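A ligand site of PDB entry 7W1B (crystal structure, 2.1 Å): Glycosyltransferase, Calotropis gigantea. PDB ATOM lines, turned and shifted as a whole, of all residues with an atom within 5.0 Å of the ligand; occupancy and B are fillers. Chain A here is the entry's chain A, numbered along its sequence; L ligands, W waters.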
ATOM      1  N   LYS A  25      17.797  -3.083 -14.041  1.00  0.00           N
ATOM      2  CA  LYS A  25      17.154  -3.464 -15.295  1.00  0.00           C
ATOM      3  C   LYS A  25      16.983  -2.277 -16.248  1.00  0.00           C
ATOM      4  O   LYS A  25      17.063  -2.462 -17.463  1.00  0.00           O
ATOM      5  CB  LYS A  25      15.793  -4.099 -15.028  1.00  0.00           C
ATOM      6  CG  LYS A  25      15.898  -5.528 -14.478  1.00  0.00           C
ATOM      7  CD  LYS A  25      14.547  -6.104 -14.113  1.00  0.00           C
ATOM      8  CE  LYS A  25      14.673  -7.061 -12.938  1.00  0.00           C
ATOM      9  NZ  LYS A  25      14.491  -8.483 -13.347  1.00  0.00           N
ATOM     10  N   GLY A  26      16.757  -1.074 -15.726  1.00  0.00           N
ATOM     11  CA  GLY A  26      16.739   0.108 -16.565  1.00  0.00           C
ATOM     12  C   GLY A  26      18.083   0.471 -17.178  1.00  0.00           C
ATOM     13  O   GLY A  26      18.122   1.346 -18.050  1.00  0.00           O
ATOM     14  N   ASN A  29      18.743  -3.422 -19.676  1.00  0.00           N
ATOM     15  CA  ASN A  29      17.908  -3.609 -20.862  1.00  0.00           C
ATOM     16  C   ASN A  29      18.344  -2.767 -22.050  1.00  0.00           C
ATOM     17  O   ASN A  29      18.482  -3.323 -23.157  1.00  0.00           O
ATOM     18  CB  ASN A  29      16.432  -3.376 -20.526  1.00  0.00           C
ATOM     19  CG  ASN A  29      15.803  -4.552 -19.800  1.00  0.00           C
ATOM     20  OD1 ASN A  29      16.445  -5.578 -19.594  1.00  0.00           O
ATOM     21  ND2 ASN A  29      14.537  -4.400 -19.387  1.00  0.00           N
ATOM     22  N   GLU A 261      11.115 -11.849 -21.868  1.00  0.00           N
ATOM     23  CA  GLU A 261      10.673 -11.536 -20.510  1.00  0.00           C
ATOM     24  C   GLU A 261       9.750 -12.637 -19.995  1.00  0.00           C
ATOM     25  O   GLU A 261       9.238 -13.455 -20.771  1.00  0.00           O
ATOM     26  CB  GLU A 261       9.960 -10.192 -20.436  1.00  0.00           C
ATOM     27  CG  GLU A 261      10.813  -8.977 -20.756  1.00  0.00           C
ATOM     28  CD  GLU A 261      11.738  -8.590 -19.627  1.00  0.00           C
ATOM     29  OE1 GLU A 261      11.738  -9.290 -18.584  1.00  0.00           O
ATOM     30  OE2 GLU A 261      12.461  -7.575 -19.780  1.00  0.00           O
ATOM     31  N   TYR A 281      -2.539  -0.036 -19.326  1.00  0.00           N
ATOM     32  CA  TYR A 281      -1.371  -0.765 -18.846  1.00  0.00           C
ATOM     33  C   TYR A 281      -0.668   0.052 -17.777  1.00  0.00           C
ATOM     34  O   TYR A 281      -0.355   1.238 -17.979  1.00  0.00           O
ATOM     35  CB  TYR A 281      -0.412  -1.090 -19.998  1.00  0.00           C
ATOM     36  CG  TYR A 281       0.956  -1.612 -19.551  1.00  0.00           C
ATOM     37  CD1 TYR A 281       1.062  -2.678 -18.666  1.00  0.00           C
ATOM     38  CD2 TYR A 281       2.126  -1.023 -20.013  1.00  0.00           C
ATOM     39  CE1 TYR A 281       2.313  -3.143 -18.251  1.00  0.00           C
ATOM     40  CE2 TYR A 281       3.364  -1.480 -19.622  1.00  0.00           C
ATOM     41  CZ  TYR A 281       3.449  -2.547 -18.744  1.00  0.00           C
ATOM     42  OH  TYR A 281       4.682  -2.995 -18.331  1.00  0.00           O
ATOM     43  N   SER A 283       2.449   0.239 -14.915  1.00  0.00           N
ATOM     44  CA  SER A 283       3.726  -0.249 -14.397  1.00  0.00           C
ATOM     45  C   SER A 283       4.528   0.899 -13.797  1.00  0.00           C
ATOM     46  O   SER A 283       4.618   1.991 -14.374  1.00  0.00           O
ATOM     47  CB  SER A 283       4.548  -0.924 -15.486  1.00  0.00           C
ATOM     48  OG  SER A 283       5.784  -1.401 -14.954  1.00  0.00           O
ATOM     49  N   PHE A 284       5.137   0.644 -12.642  1.00  0.00           N
ATOM     50  CA  PHE A 284       6.053   1.591 -12.034  1.00  0.00           C
ATOM     51  C   PHE A 284       7.494   1.110 -12.109  1.00  0.00           C
ATOM     52  O   PHE A 284       8.342   1.550 -11.318  1.00  0.00           O
ATOM     53  CB  PHE A 284       5.606   1.888 -10.604  1.00  0.00           C
ATOM     54  CG  PHE A 284       4.352   2.716 -10.551  1.00  0.00           C
ATOM     55  CD1 PHE A 284       3.122   2.126 -10.799  1.00  0.00           C
ATOM     56  CD2 PHE A 284       4.405   4.080 -10.347  1.00  0.00           C
ATOM     57  CE1 PHE A 284       1.949   2.883 -10.800  1.00  0.00           C
ATOM     58  CE2 PHE A 284       3.243   4.856 -10.339  1.00  0.00           C
ATOM     59  CZ  PHE A 284       2.018   4.255 -10.568  1.00  0.00           C
ATOM     60  N   GLY A 285       7.799   0.250 -13.077  1.00  0.00           N
ATOM     61  CA  GLY A 285       9.185  -0.112 -13.324  1.00  0.00           C
ATOM     62  C   GLY A 285       9.662  -1.196 -12.386  1.00  0.00           C
ATOM     63  O   GLY A 285       8.873  -1.864 -11.723  1.00  0.00           O
ATOM     64  N   SER A 286      10.984  -1.369 -12.324  1.00  0.00           N
ATOM     65  CA  SER A 286      11.599  -2.454 -11.558  1.00  0.00           C
ATOM     66  C   SER A 286      12.048  -2.071 -10.145  1.00  0.00           C
ATOM     67  O   SER A 286      12.312  -2.963  -9.342  1.00  0.00           O
ATOM     68  CB  SER A 286      12.801  -3.022 -12.335  1.00  0.00           C
ATOM     69  OG  SER A 286      13.839  -2.058 -12.501  1.00  0.00           O
ATOM     70  N   ILE A 287      12.131  -0.777  -9.798  1.00  0.00           N
ATOM     71  CA  ILE A 287      12.729  -0.337  -8.552  1.00  0.00           C
ATOM     72  C   ILE A 287      11.732   0.393  -7.646  1.00  0.00           C
ATOM     73  O   ILE A 287      11.722   0.175  -6.428  1.00  0.00           O
ATOM     74  CB  ILE A 287      13.958   0.558  -8.799  1.00  0.00           C
ATOM     75  CG1 ILE A 287      15.096  -0.244  -9.427  1.00  0.00           C
ATOM     76  CG2 ILE A 287      14.452   1.188  -7.496  1.00  0.00           C
ATOM     77  CD1 ILE A 287      16.329   0.568  -9.688  1.00  0.00           C
ATOM     78  N   ALA A 288      10.929   1.288  -8.206  1.00  0.00           N
ATOM     79  CA  ALA A 288      10.073   2.149  -7.390  1.00  0.00           C
ATOM     80  C   ALA A 288       9.121   1.304  -6.545  1.00  0.00           C
ATOM     81  O   ALA A 288       8.688   0.223  -6.939  1.00  0.00           O
ATOM     82  CB  ALA A 288       9.286   3.121  -8.266  1.00  0.00           C
ATOM     83  N   VAL A 312       1.162  -4.302 -13.400  1.00  0.00           N
ATOM     84  CA  VAL A 312       2.298  -5.036 -12.873  1.00  0.00           C
ATOM     85  C   VAL A 312       2.518  -4.600 -11.422  1.00  0.00           C
ATOM     86  O   VAL A 312       2.844  -3.432 -11.144  1.00  0.00           O
ATOM     87  CB  VAL A 312       3.561  -4.815 -13.708  1.00  0.00           C
ATOM     88  CG1 VAL A 312       4.699  -5.632 -13.136  1.00  0.00           C
ATOM     89  CG2 VAL A 312       3.342  -5.239 -15.132  1.00  0.00           C
ATOM     90  N   TRP A 353       5.110  -9.438 -13.443  1.00  0.00           N
ATOM     91  CA  TRP A 353       6.031  -9.000 -14.484  1.00  0.00           C
ATOM     92  C   TRP A 353       5.381  -9.297 -15.829  1.00  0.00           C
ATOM     93  O   TRP A 353       4.578 -10.228 -15.938  1.00  0.00           O
ATOM     94  CB  TRP A 353       7.380  -9.699 -14.400  1.00  0.00           C
ATOM     95  CG  TRP A 353       8.489  -8.974 -15.106  1.00  0.00           C
ATOM     96  CD1 TRP A 353       9.149  -9.368 -16.236  1.00  0.00           C
ATOM     97  CD2 TRP A 353       9.079  -7.738 -14.711  1.00  0.00           C
ATOM     98  NE1 TRP A 353      10.112  -8.447 -16.560  1.00  0.00           N
ATOM     99  CE2 TRP A 353      10.090  -7.430 -15.641  1.00  0.00           C
ATOM    100  CE3 TRP A 353       8.857  -6.849 -13.657  1.00  0.00           C
ATOM    101  CZ2 TRP A 353      10.874  -6.290 -15.552  1.00  0.00           C
ATOM    102  CZ3 TRP A 353       9.625  -5.716 -13.579  1.00  0.00           C
ATOM    103  CH2 TRP A 353      10.621  -5.444 -14.523  1.00  0.00           C
ATOM    104  N   CYS A 354       5.775  -8.545 -16.856  1.00  0.00           N
ATOM    105  CA  CYS A 354       5.214  -8.700 -18.188  1.00  0.00           C
ATOM    106  C   CYS A 354       6.295  -8.390 -19.217  1.00  0.00           C
ATOM    107  O   CYS A 354       7.302  -7.741 -18.892  1.00  0.00           O
ATOM    108  CB  CYS A 354       4.004  -7.786 -18.389  1.00  0.00           C
ATOM    109  SG  CYS A 354       4.437  -6.054 -18.776  1.00  0.00           S
ATOM    110  N   PRO A 355       6.126  -8.852 -20.472  1.00  0.00           N
ATOM    111  CA  PRO A 355       6.993  -8.369 -21.554  1.00  0.00           C
ATOM    112  C   PRO A 355       6.580  -6.968 -21.965  1.00  0.00           C
ATOM    113  O   PRO A 355       5.658  -6.792 -22.783  1.00  0.00           O
ATOM    114  CB  PRO A 355       6.747  -9.392 -22.673  1.00  0.00           C
ATOM    115  CG  PRO A 355       5.292  -9.775 -22.490  1.00  0.00           C
ATOM    116  CD  PRO A 355       5.076  -9.760 -20.971  1.00  0.00           C
ATOM    117  N   GLN A 356       7.210  -5.942 -21.382  1.00  0.00           N
ATOM    118  CA  GLN A 356       6.652  -4.589 -21.510  1.00  0.00           C
ATOM    119  C   GLN A 356       6.568  -4.145 -22.960  1.00  0.00           C
ATOM    120  O   GLN A 356       5.551  -3.579 -23.396  1.00  0.00           O
ATOM    121  CB  GLN A 356       7.485  -3.594 -20.722  1.00  0.00           C
ATOM    122  CG  GLN A 356       7.086  -2.178 -21.054  1.00  0.00           C
ATOM    123  CD  GLN A 356       7.381  -1.203 -19.957  1.00  0.00           C
ATOM    124  OE1 GLN A 356       8.155  -0.257 -20.141  1.00  0.00           O
ATOM    125  NE2 GLN A 356       6.766  -1.418 -18.800  1.00  0.00           N
ATOM    126  N   LEU A 357       7.631  -4.392 -23.742  1.00  0.00           N
ATOM    127  CA  LEU A 357       7.631  -3.921 -25.124  1.00  0.00           C
ATOM    128  C   LEU A 357       6.519  -4.573 -25.933  1.00  0.00           C
ATOM    129  O   LEU A 357       5.868  -3.926 -26.764  1.00  0.00           O
ATOM    130  CB  LEU A 357       8.997  -4.181 -25.761  1.00  0.00           C
ATOM    131  CG  LEU A 357       9.349  -3.333 -26.980  1.00  0.00           C
ATOM    132  CD1 LEU A 357       8.913  -1.882 -26.758  1.00  0.00           C
ATOM    133  CD2 LEU A 357      10.837  -3.408 -27.277  1.00  0.00           C
ATOM    134  N   HIS A 371       5.623   5.343 -14.285  1.00  0.00           N
ATOM    135  CA  HIS A 371       6.449   6.188 -13.421  1.00  0.00           C
ATOM    136  C   HIS A 371       7.409   7.080 -14.213  1.00  0.00           C
ATOM    137  O   HIS A 371       8.091   7.914 -13.612  1.00  0.00           O
ATOM    138  CB  HIS A 371       7.261   5.349 -12.438  1.00  0.00           C
ATOM    139  CG  HIS A 371       8.396   4.600 -13.055  1.00  0.00           C
ATOM    140  ND1 HIS A 371       8.238   3.814 -14.178  1.00  0.00           N
ATOM    141  CD2 HIS A 371       9.703   4.510 -12.713  1.00  0.00           C
ATOM    142  CE1 HIS A 371       9.405   3.270 -14.487  1.00  0.00           C
ATOM    143  NE2 HIS A 371      10.315   3.673 -13.616  1.00  0.00           N
ATOM    144  N   GLY A 373      10.165   6.261 -15.911  1.00  0.00           N
ATOM    145  CA  GLY A 373      11.537   5.862 -16.170  1.00  0.00           C
ATOM    146  C   GLY A 373      11.852   6.040 -17.647  1.00  0.00           C
ATOM    147  O   GLY A 373      10.960   5.984 -18.484  1.00  0.00           O
ATOM    148  N   TRP A 374      13.116   6.324 -17.978  1.00  0.00           N
ATOM    149  CA  TRP A 374      13.404   6.691 -19.362  1.00  0.00           C
ATOM    150  C   TRP A 374      13.139   5.547 -20.333  1.00  0.00           C
ATOM    151  O   TRP A 374      12.663   5.782 -21.444  1.00  0.00           O
ATOM    152  CB  TRP A 374      14.840   7.188 -19.548  1.00  0.00           C
ATOM    153  CG  TRP A 374      15.121   7.545 -21.005  1.00  0.00           C
ATOM    154  CD1 TRP A 374      16.115   7.043 -21.799  1.00  0.00           C
ATOM    155  CD2 TRP A 374      14.386   8.464 -21.835  1.00  0.00           C
ATOM    156  NE1 TRP A 374      16.046   7.590 -23.057  1.00  0.00           N
ATOM    157  CE2 TRP A 374      15.005   8.481 -23.102  1.00  0.00           C
ATOM    158  CE3 TRP A 374      13.281   9.307 -21.618  1.00  0.00           C
ATOM    159  CZ2 TRP A 374      14.548   9.273 -24.156  1.00  0.00           C
ATOM    160  CZ3 TRP A 374      12.824  10.102 -22.656  1.00  0.00           C
ATOM    161  CH2 TRP A 374      13.455  10.078 -23.918  1.00  0.00           C
ATOM    162  N   ASN A 375      13.443   4.302 -19.948  1.00  0.00           N
ATOM    163  CA  ASN A 375      13.171   3.197 -20.878  1.00  0.00           C
ATOM    164  C   ASN A 375      11.683   3.065 -21.167  1.00  0.00           C
ATOM    165  O   ASN A 375      11.273   2.905 -22.327  1.00  0.00           O
ATOM    166  CB  ASN A 375      13.705   1.875 -20.317  1.00  0.00           C
ATOM    167  CG  ASN A 375      15.203   1.832 -20.321  1.00  0.00           C
ATOM    168  OD1 ASN A 375      15.837   1.722 -21.376  1.00  0.00           O
ATOM    169  ND2 ASN A 375      15.794   1.934 -19.128  1.00  0.00           N
ATOM    170  N   SER A 376      10.850   3.125 -20.132  1.00  0.00           N
ATOM    171  CA  SER A 376       9.405   3.011 -20.330  1.00  0.00           C
ATOM    172  C   SER A 376       8.881   4.158 -21.183  1.00  0.00           C
ATOM    173  O   SER A 376       8.003   3.972 -22.021  1.00  0.00           O
ATOM    174  CB  SER A 376       8.686   2.982 -18.969  1.00  0.00           C
ATOM    175  OG  SER A 376       9.077   1.828 -18.250  1.00  0.00           O
ATOM    176  N   GLU A 379      10.236   3.488 -24.749  1.00  0.00           N
ATOM    177  CA  GLU A 379       9.498   2.343 -25.296  1.00  0.00           C
ATOM    178  C   GLU A 379       8.059   2.721 -25.634  1.00  0.00           C
ATOM    179  O   GLU A 379       7.530   2.307 -26.667  1.00  0.00           O
ATOM    180  CB  GLU A 379       9.548   1.165 -24.323  1.00  0.00           C
ATOM    181  CG  GLU A 379      10.955   0.619 -24.117  1.00  0.00           C
ATOM    182  CD  GLU A 379      11.057  -0.356 -22.970  1.00  0.00           C
ATOM    183  OE1 GLU A 379      10.036  -0.625 -22.300  1.00  0.00           O
ATOM    184  OE2 GLU A 379      12.175  -0.864 -22.743  1.00  0.00           O
ATOM    185  N   TRP A 393      10.847   9.730  -8.856  1.00  0.00           N
ATOM    186  CA  TRP A 393      12.060  10.413  -8.421  1.00  0.00           C
ATOM    187  C   TRP A 393      13.077  10.482  -9.550  1.00  0.00           C
ATOM    188  O   TRP A 393      12.855   9.970 -10.649  1.00  0.00           O
ATOM    189  CB  TRP A 393      12.679   9.761  -7.184  1.00  0.00           C
ATOM    190  CG  TRP A 393      12.428   8.287  -7.051  1.00  0.00           C
ATOM    191  CD1 TRP A 393      11.543   7.680  -6.200  1.00  0.00           C
ATOM    192  CD2 TRP A 393      13.067   7.241  -7.784  1.00  0.00           C
ATOM    193  NE1 TRP A 393      11.603   6.313  -6.361  1.00  0.00           N
ATOM    194  CE2 TRP A 393      12.525   6.013  -7.331  1.00  0.00           C
ATOM    195  CE3 TRP A 393      14.065   7.216  -8.780  1.00  0.00           C
ATOM    196  CZ2 TRP A 393      12.924   4.777  -7.841  1.00  0.00           C
ATOM    197  CZ3 TRP A 393      14.451   5.983  -9.290  1.00  0.00           C
ATOM    198  CH2 TRP A 393      13.891   4.783  -8.811  1.00  0.00           C
ATOM    199  N   GLN A 396      12.440  11.068 -13.449  1.00  0.00           N
ATOM    200  CA  GLN A 396      11.058  10.781 -13.817  1.00  0.00           C
ATOM    201  C   GLN A 396      10.224  12.051 -13.857  1.00  0.00           C
ATOM    202  O   GLN A 396       9.321  12.178 -14.693  1.00  0.00           O
ATOM    203  CB  GLN A 396      10.468   9.758 -12.853  1.00  0.00           C
ATOM    204  CG  GLN A 396      11.116   8.372 -12.975  1.00  0.00           C
ATOM    205  CD  GLN A 396      11.088   7.592 -11.667  1.00  0.00           C
ATOM    206  OE1 GLN A 396      10.207   7.792 -10.825  1.00  0.00           O
ATOM    207  NE2 GLN A 396      12.032   6.677 -11.510  1.00  0.00           N
HETATM  208  N1  LIG L   1       9.885  -3.938 -17.736  1.00  0.00           N
HETATM  209  C1  LIG L   1       9.425  -5.113 -18.149  1.00  0.00           C
HETATM  210  N2  LIG L   1       8.342  -5.659 -17.632  1.00  0.00           N
HETATM  211  C2  LIG L   1       7.683  -5.024 -16.676  1.00  0.00           C
HETATM  212  C3  LIG L   1       8.124  -3.796 -16.195  1.00  0.00           C
HETATM  213  C4  LIG L   1       9.277  -3.273 -16.777  1.00  0.00           C
HETATM  214  O1  LIG L   1      10.091  -5.792 -19.181  1.00  0.00           O
HETATM  215  O2  LIG L   1       6.568  -5.616 -16.143  1.00  0.00           O
HETATM  216  C5  LIG L   1      11.124  -3.391 -18.344  1.00  0.00           C
HETATM  217  C6  LIG L   1      10.864  -2.130 -19.196  1.00  0.00           C
HETATM  218  O3  LIG L   1      10.677  -2.548 -20.468  1.00  0.00           O
HETATM  219  C7  LIG L   1      12.177  -1.338 -19.035  1.00  0.00           C
HETATM  220  C8  LIG L   1      12.605  -1.612 -17.816  1.00  0.00           C
HETATM  221  O4  LIG L   1      11.937  -3.017 -17.395  1.00  0.00           O
HETATM  222  O5  LIG L   1      13.144  -1.869 -20.063  1.00  0.00           O
HETATM  223  C9  LIG L   1      12.196  -0.555 -16.796  1.00  0.00           C
HETATM  224  O6  LIG L   1      13.089   0.508 -16.940  1.00  0.00           O
HETATM  225  P1  LIG L   1      12.685   2.079 -16.668  1.00  0.00           P
HETATM  226  O7  LIG L   1      11.397   2.456 -17.341  1.00  0.00           O
HETATM  227  O8  LIG L   1      13.785   2.995 -17.199  1.00  0.00           O
HETATM  228  O9  LIG L   1      12.513   2.345 -15.045  1.00  0.00           O
HETATM  229  P2  LIG L   1      13.320   1.668 -13.767  1.00  0.00           P
HETATM  230  O10 LIG L   1      12.853   2.488 -12.586  1.00  0.00           O
HETATM  231  O11 LIG L   1      12.982   0.230 -13.606  1.00  0.00           O
HETATM  232  O12 LIG L   1      14.808   1.783 -13.918  1.00  0.00           O
HETATM  233  O   HOH W   1      11.153   1.628 -10.854  1.00  0.00           O
HETATM  234  O   HOH W   2      14.736   4.208 -12.116  1.00  0.00           O
HETATM  235  O   HOH W   3       7.751  -0.263 -16.564  1.00  0.00           O
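The side-chain sulfur (SG) of Cys 354 lies within hydrogen-bond range of an oxygen (O2) of the ligand (3.4 Å).
The backbone NH (N) of Cys 354 is in hydrogen-bond range of an oxygen (O2) of the ligand, 3.1 Å away.
An oxygen (O3) of the ligand sits close to the side-chain amide oxygen (OE1) of Gln 356 (3.4 Å).
The side-chain carboxylate (OE1) of Glu 379 lies within hydrogen-bond range of an oxygen (O3) of the ligand, 2.7 Å away.
The side-chain amide nitrogen (ND2) of Asn 375 lies within hydrogen-bond range of an oxygen (O8) of the ligand (3.0 Å).
O8 of the ligand lies within hydrogen-bond range of N of Asn 375 (3.1 Å).
The side-chain hydroxyl (OG) of Ser 376 lies within hydrogen-bond range of an oxygen (O7) of the ligand, 2.6 Å away.
O5 of the ligand is in hydrogen-bond range of ND2 of Asn 29 (3.0 Å).
The side-chain hydroxyl of Ser 286 is in hydrogen-bond range of an oxygen (O11) of the ligand (2.7 Å).
O of Cys 354 lies within hydrogen-bond range of N2 of the ligand (2.6 Å).
N of Trp 374 lies within hydrogen-bond range of O8 of the ligand (3.5 Å).
The backbone NH (N) of Ser 376 sits at hydrogen-bond distance from an oxygen (O7) of the ligand.
The backbone NH (N) of Ser 286 lies within hydrogen-bond range of an oxygen (O11) of the ligand, at 2.9 Å.
O9 of the ligand lies within hydrogen-bond range of NE2 of His 371 (2.9 Å).
The side-chain amide oxygen of Gln 356 lies close to the side-chain carboxylate of Glu 379, at 2.9 Å.
A ring nitrogen (NE2) of His 371 sits close to the backbone NH (N) of Gly 373, at 3.5 Å.
The side-chain carboxylate (OE1) of Glu 261 is in hydrogen-bond range of the indole nitrogen (NE1) of Trp 353 (2.7 Å).
OG of Ser 376 sits at hydrogen-bond distance from OE1 of Gln 356, at 3.0 Å.
The side-chain hydroxyl of Ser 283 is in hydrogen-bond range of the backbone NH of Gly 285, at 3.2 Å.
ND2 of Asn 375 sits at hydrogen-bond distance from O of Gly 26 (2.6 Å).
OH of Tyr 281 is in hydrogen-bond range of NE2 of Gln 356, at 2.7 Å.
N of His 371 is in hydrogen-bond range of O of Ser 283 (3.5 Å).
OE2 of Glu 261 lies close to O1 of the ligand (3.0 Å).
NE1 of Trp 353 sits close to N2 of the ligand.
Gly 26 touches the ligand.
Tyr 281 touches the ligand.
Ser 283 touches the ligand (OG to C3, 3.6 Å).
C of Gly 285 touches O11 of the ligand, at 3.8 Å.
Val 312 touches the ligand.
Gly 373 touches the ligand (CA to O7, 3.6 Å).
Hydrophobic or aromatic side chains within 4 Å of the ligand: Val 312, Trp 353 and His 371.
17 residues have an atom within 4 Å of the ligand: Gly 26, Asn 29, Glu 261, Tyr 281, Ser 283, Gly 285, Ser 286, Val 312, Trp 353, Cys 354, Gln 356, His 371, Gly 373, Trp 374, Asn 375, Ser 376 and Glu 379.
Water W3 lies within hydrogen-bond range of the side-chain amide nitrogen (NE2) of Gln 356 (2.7 Å), the side-chain hydroxyl (OG) of Ser 283 (2.8 Å) and the side-chain hydroxyl (OG) of Ser 376 (3.0 Å).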
